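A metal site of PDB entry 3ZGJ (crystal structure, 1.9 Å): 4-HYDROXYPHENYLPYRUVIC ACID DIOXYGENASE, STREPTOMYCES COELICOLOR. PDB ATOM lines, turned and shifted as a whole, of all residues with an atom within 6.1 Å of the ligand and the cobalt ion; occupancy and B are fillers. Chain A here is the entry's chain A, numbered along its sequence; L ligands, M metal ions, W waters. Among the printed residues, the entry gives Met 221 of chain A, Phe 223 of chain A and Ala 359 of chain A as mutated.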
ATOM      1  N   HIS A 181      16.434 -12.998 -11.253  1.00  0.00           N
ATOM      2  CA  HIS A 181      17.848 -12.685 -11.076  1.00  0.00           C
ATOM      3  C   HIS A 181      18.499 -13.833 -10.312  1.00  0.00           C
ATOM      4  O   HIS A 181      17.787 -14.724  -9.706  1.00  0.00           O
ATOM      5  CB  HIS A 181      18.015 -11.353 -10.275  1.00  0.00           C
ATOM      6  CG  HIS A 181      17.470 -11.385  -8.869  1.00  0.00           C
ATOM      7  ND1 HIS A 181      16.184 -11.002  -8.549  1.00  0.00           N
ATOM      8  CD2 HIS A 181      18.077 -11.691  -7.694  1.00  0.00           C
ATOM      9  CE1 HIS A 181      16.010 -11.080  -7.225  1.00  0.00           C
ATOM     10  NE2 HIS A 181      17.150 -11.493  -6.686  1.00  0.00           N
ATOM     11  N   VAL A 182      19.823 -13.871 -10.426  1.00  0.00           N
ATOM     12  CA  VAL A 182      20.628 -14.847  -9.717  1.00  0.00           C
ATOM     13  C   VAL A 182      21.514 -14.044  -8.752  1.00  0.00           C
ATOM     14  O   VAL A 182      22.137 -13.067  -9.200  1.00  0.00           O
ATOM     15  CB  VAL A 182      21.494 -15.624 -10.694  1.00  0.00           C
ATOM     16  CG1 VAL A 182      22.519 -16.547  -9.981  1.00  0.00           C
ATOM     17  CG2 VAL A 182      20.598 -16.430 -11.713  1.00  0.00           C
ATOM     18  N   ALA A 183      21.616 -14.488  -7.493  1.00  0.00           N
ATOM     19  CA  ALA A 183      22.458 -13.796  -6.463  1.00  0.00           C
ATOM     20  C   ALA A 183      23.699 -14.632  -6.222  1.00  0.00           C
ATOM     21  O   ALA A 183      23.634 -15.885  -6.122  1.00  0.00           O
ATOM     22  CB  ALA A 183      21.645 -13.477  -5.184  1.00  0.00           C
ATOM     23  N   MET A 219      27.596  -5.802   3.842  1.00  0.00           N
ATOM     24  CA  MET A 219      27.926  -6.396   2.558  1.00  0.00           C
ATOM     25  C   MET A 219      27.777  -5.353   1.489  1.00  0.00           C
ATOM     26  O   MET A 219      26.954  -4.471   1.574  1.00  0.00           O
ATOM     27  CB  MET A 219      27.002  -7.589   2.264  1.00  0.00           C
ATOM     28  CG  MET A 219      25.557  -7.187   2.309  1.00  0.00           C
ATOM     29  SD  MET A 219      24.427  -8.636   2.369  1.00  0.00           S
ATOM     30  CE  MET A 219      24.506  -9.025   4.108  1.00  0.00           C
ATOM     31  N   MET A 221      27.139  -4.821  -2.555  1.00  0.00           N
ATOM     32  CA  MET A 221      26.671  -5.516  -3.737  1.00  0.00           C
ATOM     33  C   MET A 221      26.512  -4.611  -4.946  1.00  0.00           C
ATOM     34  O   MET A 221      26.289  -3.405  -4.823  1.00  0.00           O
ATOM     35  CB  MET A 221      25.376  -6.261  -3.366  1.00  0.00           C
ATOM     36  CG  MET A 221      24.148  -5.412  -3.190  1.00  0.00           C
ATOM     37  SD  MET A 221      22.795  -6.326  -2.378  1.00  0.00           S
ATOM     38  CE  MET A 221      23.531  -6.621  -0.785  1.00  0.00           C
ATOM     39  N   PHE A 223      24.286  -4.878  -8.625  1.00  0.00           N
ATOM     40  CA  PHE A 223      23.377  -5.598  -9.528  1.00  0.00           C
ATOM     41  C   PHE A 223      23.883  -5.297 -10.934  1.00  0.00           C
ATOM     42  O   PHE A 223      24.144  -4.078 -11.238  1.00  0.00           O
ATOM     43  CB  PHE A 223      21.952  -5.140  -9.333  1.00  0.00           C
ATOM     44  CG  PHE A 223      21.373  -5.487  -7.991  1.00  0.00           C
ATOM     45  CD1 PHE A 223      21.658  -4.709  -6.861  1.00  0.00           C
ATOM     46  CD2 PHE A 223      20.517  -6.598  -7.849  1.00  0.00           C
ATOM     47  CE1 PHE A 223      21.116  -5.032  -5.605  1.00  0.00           C
ATOM     48  CE2 PHE A 223      19.966  -6.909  -6.612  1.00  0.00           C
ATOM     49  CZ  PHE A 223      20.271  -6.121  -5.478  1.00  0.00           C
ATOM     50  N   THR A 234      22.948 -10.448  -9.003  1.00  0.00           N
ATOM     51  CA  THR A 234      23.403  -9.700  -7.806  1.00  0.00           C
ATOM     52  C   THR A 234      24.759 -10.213  -7.457  1.00  0.00           C
ATOM     53  O   THR A 234      24.921 -11.432  -7.160  1.00  0.00           O
ATOM     54  CB  THR A 234      22.524  -9.907  -6.585  1.00  0.00           C
ATOM     55  OG1 THR A 234      21.181  -9.798  -6.959  1.00  0.00           O
ATOM     56  CG2 THR A 234      22.863  -8.778  -5.484  1.00  0.00           C
ATOM     57  N   ILE A 236      27.572 -10.039  -4.730  1.00  0.00           N
ATOM     58  CA  ILE A 236      27.622  -9.693  -3.292  1.00  0.00           C
ATOM     59  C   ILE A 236      28.996 -10.097  -2.716  1.00  0.00           C
ATOM     60  O   ILE A 236      29.457 -11.255  -2.856  1.00  0.00           O
ATOM     61  CB  ILE A 236      26.548 -10.459  -2.469  1.00  0.00           C
ATOM     62  CG1 ILE A 236      25.154 -10.306  -3.111  1.00  0.00           C
ATOM     63  CG2 ILE A 236      26.555  -9.992  -1.020  1.00  0.00           C
ATOM     64  CD1 ILE A 236      24.234 -11.509  -2.880  1.00  0.00           C
ATOM     65  N   GLN A 246      26.804 -13.324   7.388  1.00  0.00           N
ATOM     66  CA  GLN A 246      26.119 -14.361   6.588  1.00  0.00           C
ATOM     67  C   GLN A 246      26.820 -14.610   5.223  1.00  0.00           C
ATOM     68  O   GLN A 246      26.819 -15.741   4.725  1.00  0.00           O
ATOM     69  CB  GLN A 246      24.676 -13.942   6.431  1.00  0.00           C
ATOM     70  CG  GLN A 246      24.480 -12.709   5.537  1.00  0.00           C
ATOM     71  CD  GLN A 246      23.048 -12.218   5.626  1.00  0.00           C
ATOM     72  OE1 GLN A 246      22.376 -12.065   4.627  1.00  0.00           O
ATOM     73  NE2 GLN A 246      22.556 -12.012   6.837  1.00  0.00           N
ATOM     74  N   ILE A 247      27.444 -13.586   4.600  1.00  0.00           N
ATOM     75  CA  ILE A 247      28.111 -13.843   3.347  1.00  0.00           C
ATOM     76  C   ILE A 247      29.369 -14.623   3.562  1.00  0.00           C
ATOM     77  O   ILE A 247      29.731 -15.507   2.780  1.00  0.00           O
ATOM     78  CB  ILE A 247      28.408 -12.567   2.520  1.00  0.00           C
ATOM     79  CG1 ILE A 247      27.138 -11.738   2.421  1.00  0.00           C
ATOM     80  CG2 ILE A 247      29.002 -12.913   1.138  1.00  0.00           C
ATOM     81  CD1 ILE A 247      25.885 -12.439   1.811  1.00  0.00           C
ATOM     82  N   GLN A 260      24.053 -18.059  -4.308  1.00  0.00           N
ATOM     83  CA  GLN A 260      23.387 -18.064  -3.031  1.00  0.00           C
ATOM     84  C   GLN A 260      21.888 -18.227  -3.199  1.00  0.00           C
ATOM     85  O   GLN A 260      21.243 -18.821  -2.317  1.00  0.00           O
ATOM     86  CB  GLN A 260      23.552 -16.678  -2.380  1.00  0.00           C
ATOM     87  CG  GLN A 260      23.126 -16.649  -0.896  1.00  0.00           C
ATOM     88  CD  GLN A 260      22.735 -15.218  -0.444  1.00  0.00           C
ATOM     89  OE1 GLN A 260      22.043 -14.487  -1.145  1.00  0.00           O
ATOM     90  NE2 GLN A 260      23.160 -14.853   0.753  1.00  0.00           N
ATOM     91  N   HIS A 261      21.304 -17.590  -4.213  1.00  0.00           N
ATOM     92  CA  HIS A 261      19.842 -17.767  -4.468  1.00  0.00           C
ATOM     93  C   HIS A 261      19.419 -17.522  -5.896  1.00  0.00           C
ATOM     94  O   HIS A 261      20.052 -16.737  -6.603  1.00  0.00           O
ATOM     95  CB  HIS A 261      18.926 -16.996  -3.483  1.00  0.00           C
ATOM     96  CG  HIS A 261      18.892 -15.488  -3.619  1.00  0.00           C
ATOM     97  ND1 HIS A 261      19.669 -14.669  -2.815  1.00  0.00           N
ATOM     98  CD2 HIS A 261      18.106 -14.651  -4.354  1.00  0.00           C
ATOM     99  CE1 HIS A 261      19.361 -13.398  -3.048  1.00  0.00           C
ATOM    100  NE2 HIS A 261      18.425 -13.348  -3.983  1.00  0.00           N
ATOM    101  N   ALA A 263      15.969 -16.300  -7.956  1.00  0.00           N
ATOM    102  CA  ALA A 263      14.681 -15.644  -7.646  1.00  0.00           C
ATOM    103  C   ALA A 263      13.733 -15.843  -8.761  1.00  0.00           C
ATOM    104  O   ALA A 263      14.054 -15.554  -9.955  1.00  0.00           O
ATOM    105  CB  ALA A 263      14.921 -14.100  -7.439  1.00  0.00           C
ATOM    106  N   GLN A 325       8.915  -9.345  -1.899  1.00  0.00           N
ATOM    107  CA  GLN A 325       9.937 -10.412  -1.949  1.00  0.00           C
ATOM    108  C   GLN A 325       9.853 -11.284  -0.692  1.00  0.00           C
ATOM    109  O   GLN A 325       9.446 -10.802   0.376  1.00  0.00           O
ATOM    110  CB  GLN A 325      11.348  -9.781  -2.039  1.00  0.00           C
ATOM    111  CG  GLN A 325      11.711  -9.185  -3.388  1.00  0.00           C
ATOM    112  CD  GLN A 325      13.045  -8.396  -3.292  1.00  0.00           C
ATOM    113  OE1 GLN A 325      13.057  -7.296  -2.750  1.00  0.00           O
ATOM    114  NE2 GLN A 325      14.141  -8.942  -3.823  1.00  0.00           N
ATOM    115  N   PHE A 327      12.220 -14.964   0.994  1.00  0.00           N
ATOM    116  CA  PHE A 327      13.148 -16.016   0.886  1.00  0.00           C
ATOM    117  C   PHE A 327      12.609 -17.299   1.544  1.00  0.00           C
ATOM    118  O   PHE A 327      11.964 -17.279   2.631  1.00  0.00           O
ATOM    119  CB  PHE A 327      14.443 -15.684   1.678  1.00  0.00           C
ATOM    120  CG  PHE A 327      15.346 -14.660   1.026  1.00  0.00           C
ATOM    121  CD1 PHE A 327      15.163 -14.254  -0.306  1.00  0.00           C
ATOM    122  CD2 PHE A 327      16.453 -14.156   1.759  1.00  0.00           C
ATOM    123  CE1 PHE A 327      16.045 -13.319  -0.898  1.00  0.00           C
ATOM    124  CE2 PHE A 327      17.337 -13.257   1.167  1.00  0.00           C
ATOM    125  CZ  PHE A 327      17.142 -12.828  -0.180  1.00  0.00           C
ATOM    126  N   GLU A 340      14.119 -17.457  -3.817  1.00  0.00           N
ATOM    127  CA  GLU A 340      13.400 -16.247  -3.572  1.00  0.00           C
ATOM    128  C   GLU A 340      12.276 -16.200  -4.500  1.00  0.00           C
ATOM    129  O   GLU A 340      12.408 -16.620  -5.687  1.00  0.00           O
ATOM    130  CB  GLU A 340      14.283 -15.006  -3.897  1.00  0.00           C
ATOM    131  CG  GLU A 340      13.530 -13.679  -3.870  1.00  0.00           C
ATOM    132  CD  GLU A 340      14.383 -12.494  -4.323  1.00  0.00           C
ATOM    133  OE1 GLU A 340      15.604 -12.613  -4.253  1.00  0.00           O
ATOM    134  OE2 GLU A 340      13.835 -11.500  -4.807  1.00  0.00           O
ATOM    135  N   PHE A 350      15.528  -2.768  -7.579  1.00  0.00           N
ATOM    136  CA  PHE A 350      15.542  -3.412  -6.271  1.00  0.00           C
ATOM    137  C   PHE A 350      15.475  -2.339  -5.219  1.00  0.00           C
ATOM    138  O   PHE A 350      15.927  -1.248  -5.463  1.00  0.00           O
ATOM    139  CB  PHE A 350      16.785  -4.295  -6.134  1.00  0.00           C
ATOM    140  CG  PHE A 350      16.869  -5.375  -7.198  1.00  0.00           C
ATOM    141  CD1 PHE A 350      16.201  -6.611  -7.036  1.00  0.00           C
ATOM    142  CD2 PHE A 350      17.570  -5.157  -8.398  1.00  0.00           C
ATOM    143  CE1 PHE A 350      16.258  -7.593  -8.043  1.00  0.00           C
ATOM    144  CE2 PHE A 350      17.616  -6.121  -9.399  1.00  0.00           C
ATOM    145  CZ  PHE A 350      16.974  -7.356  -9.216  1.00  0.00           C
ATOM    146  N   GLY A 351      14.941  -2.646  -4.042  1.00  0.00           N
ATOM    147  CA  GLY A 351      14.727  -1.613  -3.033  1.00  0.00           C
ATOM    148  C   GLY A 351      15.655  -1.893  -1.859  1.00  0.00           C
ATOM    149  O   GLY A 351      15.758  -3.032  -1.407  1.00  0.00           O
ATOM    150  N   ASN A 354      13.853  -3.532   1.251  1.00  0.00           N
ATOM    151  CA  ASN A 354      13.713  -5.038   1.159  1.00  0.00           C
ATOM    152  C   ASN A 354      15.016  -5.771   1.325  1.00  0.00           C
ATOM    153  O   ASN A 354      15.081  -6.783   2.028  1.00  0.00           O
ATOM    154  CB  ASN A 354      13.134  -5.447  -0.186  1.00  0.00           C
ATOM    155  CG  ASN A 354      11.615  -5.411  -0.188  1.00  0.00           C
ATOM    156  OD1 ASN A 354      10.983  -5.073   0.818  1.00  0.00           O
ATOM    157  ND2 ASN A 354      11.027  -5.746  -1.338  1.00  0.00           N
ATOM    158  N   ILE A 355      16.087  -5.273   0.689  1.00  0.00           N
ATOM    159  CA  ILE A 355      17.389  -5.951   0.787  1.00  0.00           C
ATOM    160  C   ILE A 355      17.791  -6.089   2.275  1.00  0.00           C
ATOM    161  O   ILE A 355      18.180  -7.160   2.789  1.00  0.00           O
ATOM    162  CB  ILE A 355      18.453  -5.237  -0.049  1.00  0.00           C
ATOM    163  CG1 ILE A 355      18.035  -5.217  -1.558  1.00  0.00           C
ATOM    164  CG2 ILE A 355      19.852  -5.814   0.211  1.00  0.00           C
ATOM    165  CD1 ILE A 355      18.951  -4.398  -2.472  1.00  0.00           C
ATOM    166  N   LYS A 356      17.662  -5.000   3.009  1.00  0.00           N
ATOM    167  CA  LYS A 356      18.021  -5.017   4.425  1.00  0.00           C
ATOM    168  C   LYS A 356      17.131  -5.983   5.237  1.00  0.00           C
ATOM    169  O   LYS A 356      17.631  -6.769   6.056  1.00  0.00           O
ATOM    170  CB  LYS A 356      17.909  -3.611   5.027  1.00  0.00           C
ATOM    171  CG  LYS A 356      18.465  -3.477   6.454  1.00  0.00           C
ATOM    172  CD  LYS A 356      17.998  -2.112   6.970  1.00  0.00           C
ATOM    173  CE  LYS A 356      18.471  -1.802   8.391  1.00  0.00           C
ATOM    174  NZ  LYS A 356      19.914  -2.156   8.535  1.00  0.00           N
ATOM    175  N   LEU A 358      15.397  -8.552   4.115  1.00  0.00           N
ATOM    176  CA  LEU A 358      15.757  -9.930   3.719  1.00  0.00           C
ATOM    177  C   LEU A 358      17.000 -10.375   4.448  1.00  0.00           C
ATOM    178  O   LEU A 358      17.078 -11.510   4.943  1.00  0.00           O
ATOM    179  CB  LEU A 358      16.055  -9.989   2.205  1.00  0.00           C
ATOM    180  CG  LEU A 358      14.747  -9.907   1.399  1.00  0.00           C
ATOM    181  CD1 LEU A 358      14.981  -9.388  -0.034  1.00  0.00           C
ATOM    182  CD2 LEU A 358      13.982 -11.284   1.409  1.00  0.00           C
ATOM    183  N   ALA A 359      18.013  -9.504   4.502  1.00  0.00           N
ATOM    184  CA  ALA A 359      19.300  -9.875   5.075  1.00  0.00           C
ATOM    185  C   ALA A 359      19.109 -10.033   6.604  1.00  0.00           C
ATOM    186  O   ALA A 359      19.724 -10.858   7.248  1.00  0.00           O
ATOM    187  CB  ALA A 359      20.311  -8.753   4.750  1.00  0.00           C
HETATM  188  C1  LIG L   1      19.591  -9.624  -2.412  1.00  0.00           C
HETATM  189  C2  LIG L   1      20.921  -9.963  -2.151  1.00  0.00           C
HETATM  190  C3  LIG L   1      21.346 -10.174  -0.848  1.00  0.00           C
HETATM  191  C4  LIG L   1      20.488 -10.080   0.247  1.00  0.00           C
HETATM  192  C5  LIG L   1      19.173  -9.720   0.002  1.00  0.00           C
HETATM  193  C6  LIG L   1      18.721  -9.512  -1.312  1.00  0.00           C
HETATM  194  C7  LIG L   1      19.120  -9.420  -3.758  1.00  0.00           C
HETATM  195  C8  LIG L   1      17.629  -9.020  -3.776  1.00  0.00           C
HETATM  196  O1  LIG L   1      19.433 -10.530  -4.673  1.00  0.00           O
HETATM  197  O2  LIG L   1      17.347  -7.789  -3.833  1.00  0.00           O
HETATM  198  O3  LIG L   1      16.792  -9.922  -3.640  1.00  0.00           O
HETATM  199 CO    CO M   1      17.369 -11.634  -4.620  1.00  0.00          CO
HETATM  200  O   HOH W   1      14.906  -5.496  -3.560  1.00  0.00           O
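The side-chain amide nitrogen (NE2) of Gln 325 sits at hydrogen-bond distance from an oxygen (O2) of the ligand (3.4 Å).
O1 of the ligand sits close to OG1 of Thr 234 (3.0 Å).
The backbone NH (N) of Ala 183 is in hydrogen-bond range of the backbone carbonyl oxygen (O) of His 261, 2.9 Å away.
The side-chain amide oxygen (OE1) of Gln 325 is in hydrogen-bond range of the side-chain amide nitrogen (ND2) of Asn 354, at 2.9 Å.
A ring nitrogen (ND1) of His 261 sits at hydrogen-bond distance from the side-chain amide oxygen (OE1) of Gln 260 (2.9 Å).
The backbone NH of Thr 234 lies within hydrogen-bond range of the backbone carbonyl oxygen of Val 182 (2.7 Å).
The side-chain carboxylate of Glu 340 sits at hydrogen-bond distance from the side-chain amide nitrogen of Gln 325 (2.8 Å).
The backbone carbonyl oxygen (O) of His 181 sits at hydrogen-bond distance from the backbone NH (N) of Ala 263.
The backbone carbonyl oxygen (O) of Ala 183 lies within hydrogen-bond range of the backbone NH (N) of Gln 260.
Residues that only touch the ligand: Ile 355, Phe 350, Phe 327, Ala 183, Ile 236, Phe 223 and Leu 358.
Of the 23 residues printed, 12 come within 4 Å of the ligand.
Three residues have an atom within 4 Å of the cobalt ion: His 181, His 261 and Glu 340.
The cobalt ion is bound by OE1 of Glu 340 (2.1 Å), O3 of the ligand (2.1 Å), NE2 of His 181 (2.1 Å), NE2 of His 261 (2.1 Å) and O1 of the ligand (2.3 Å).
Water W1 lies within hydrogen-bond range of the side-chain amide oxygen (OE1) of Gln 325 (2.7 Å), the backbone NH (N) of Gly 351 (2.9 Å) and an oxygen (O2) of the ligand (3.4 Å).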
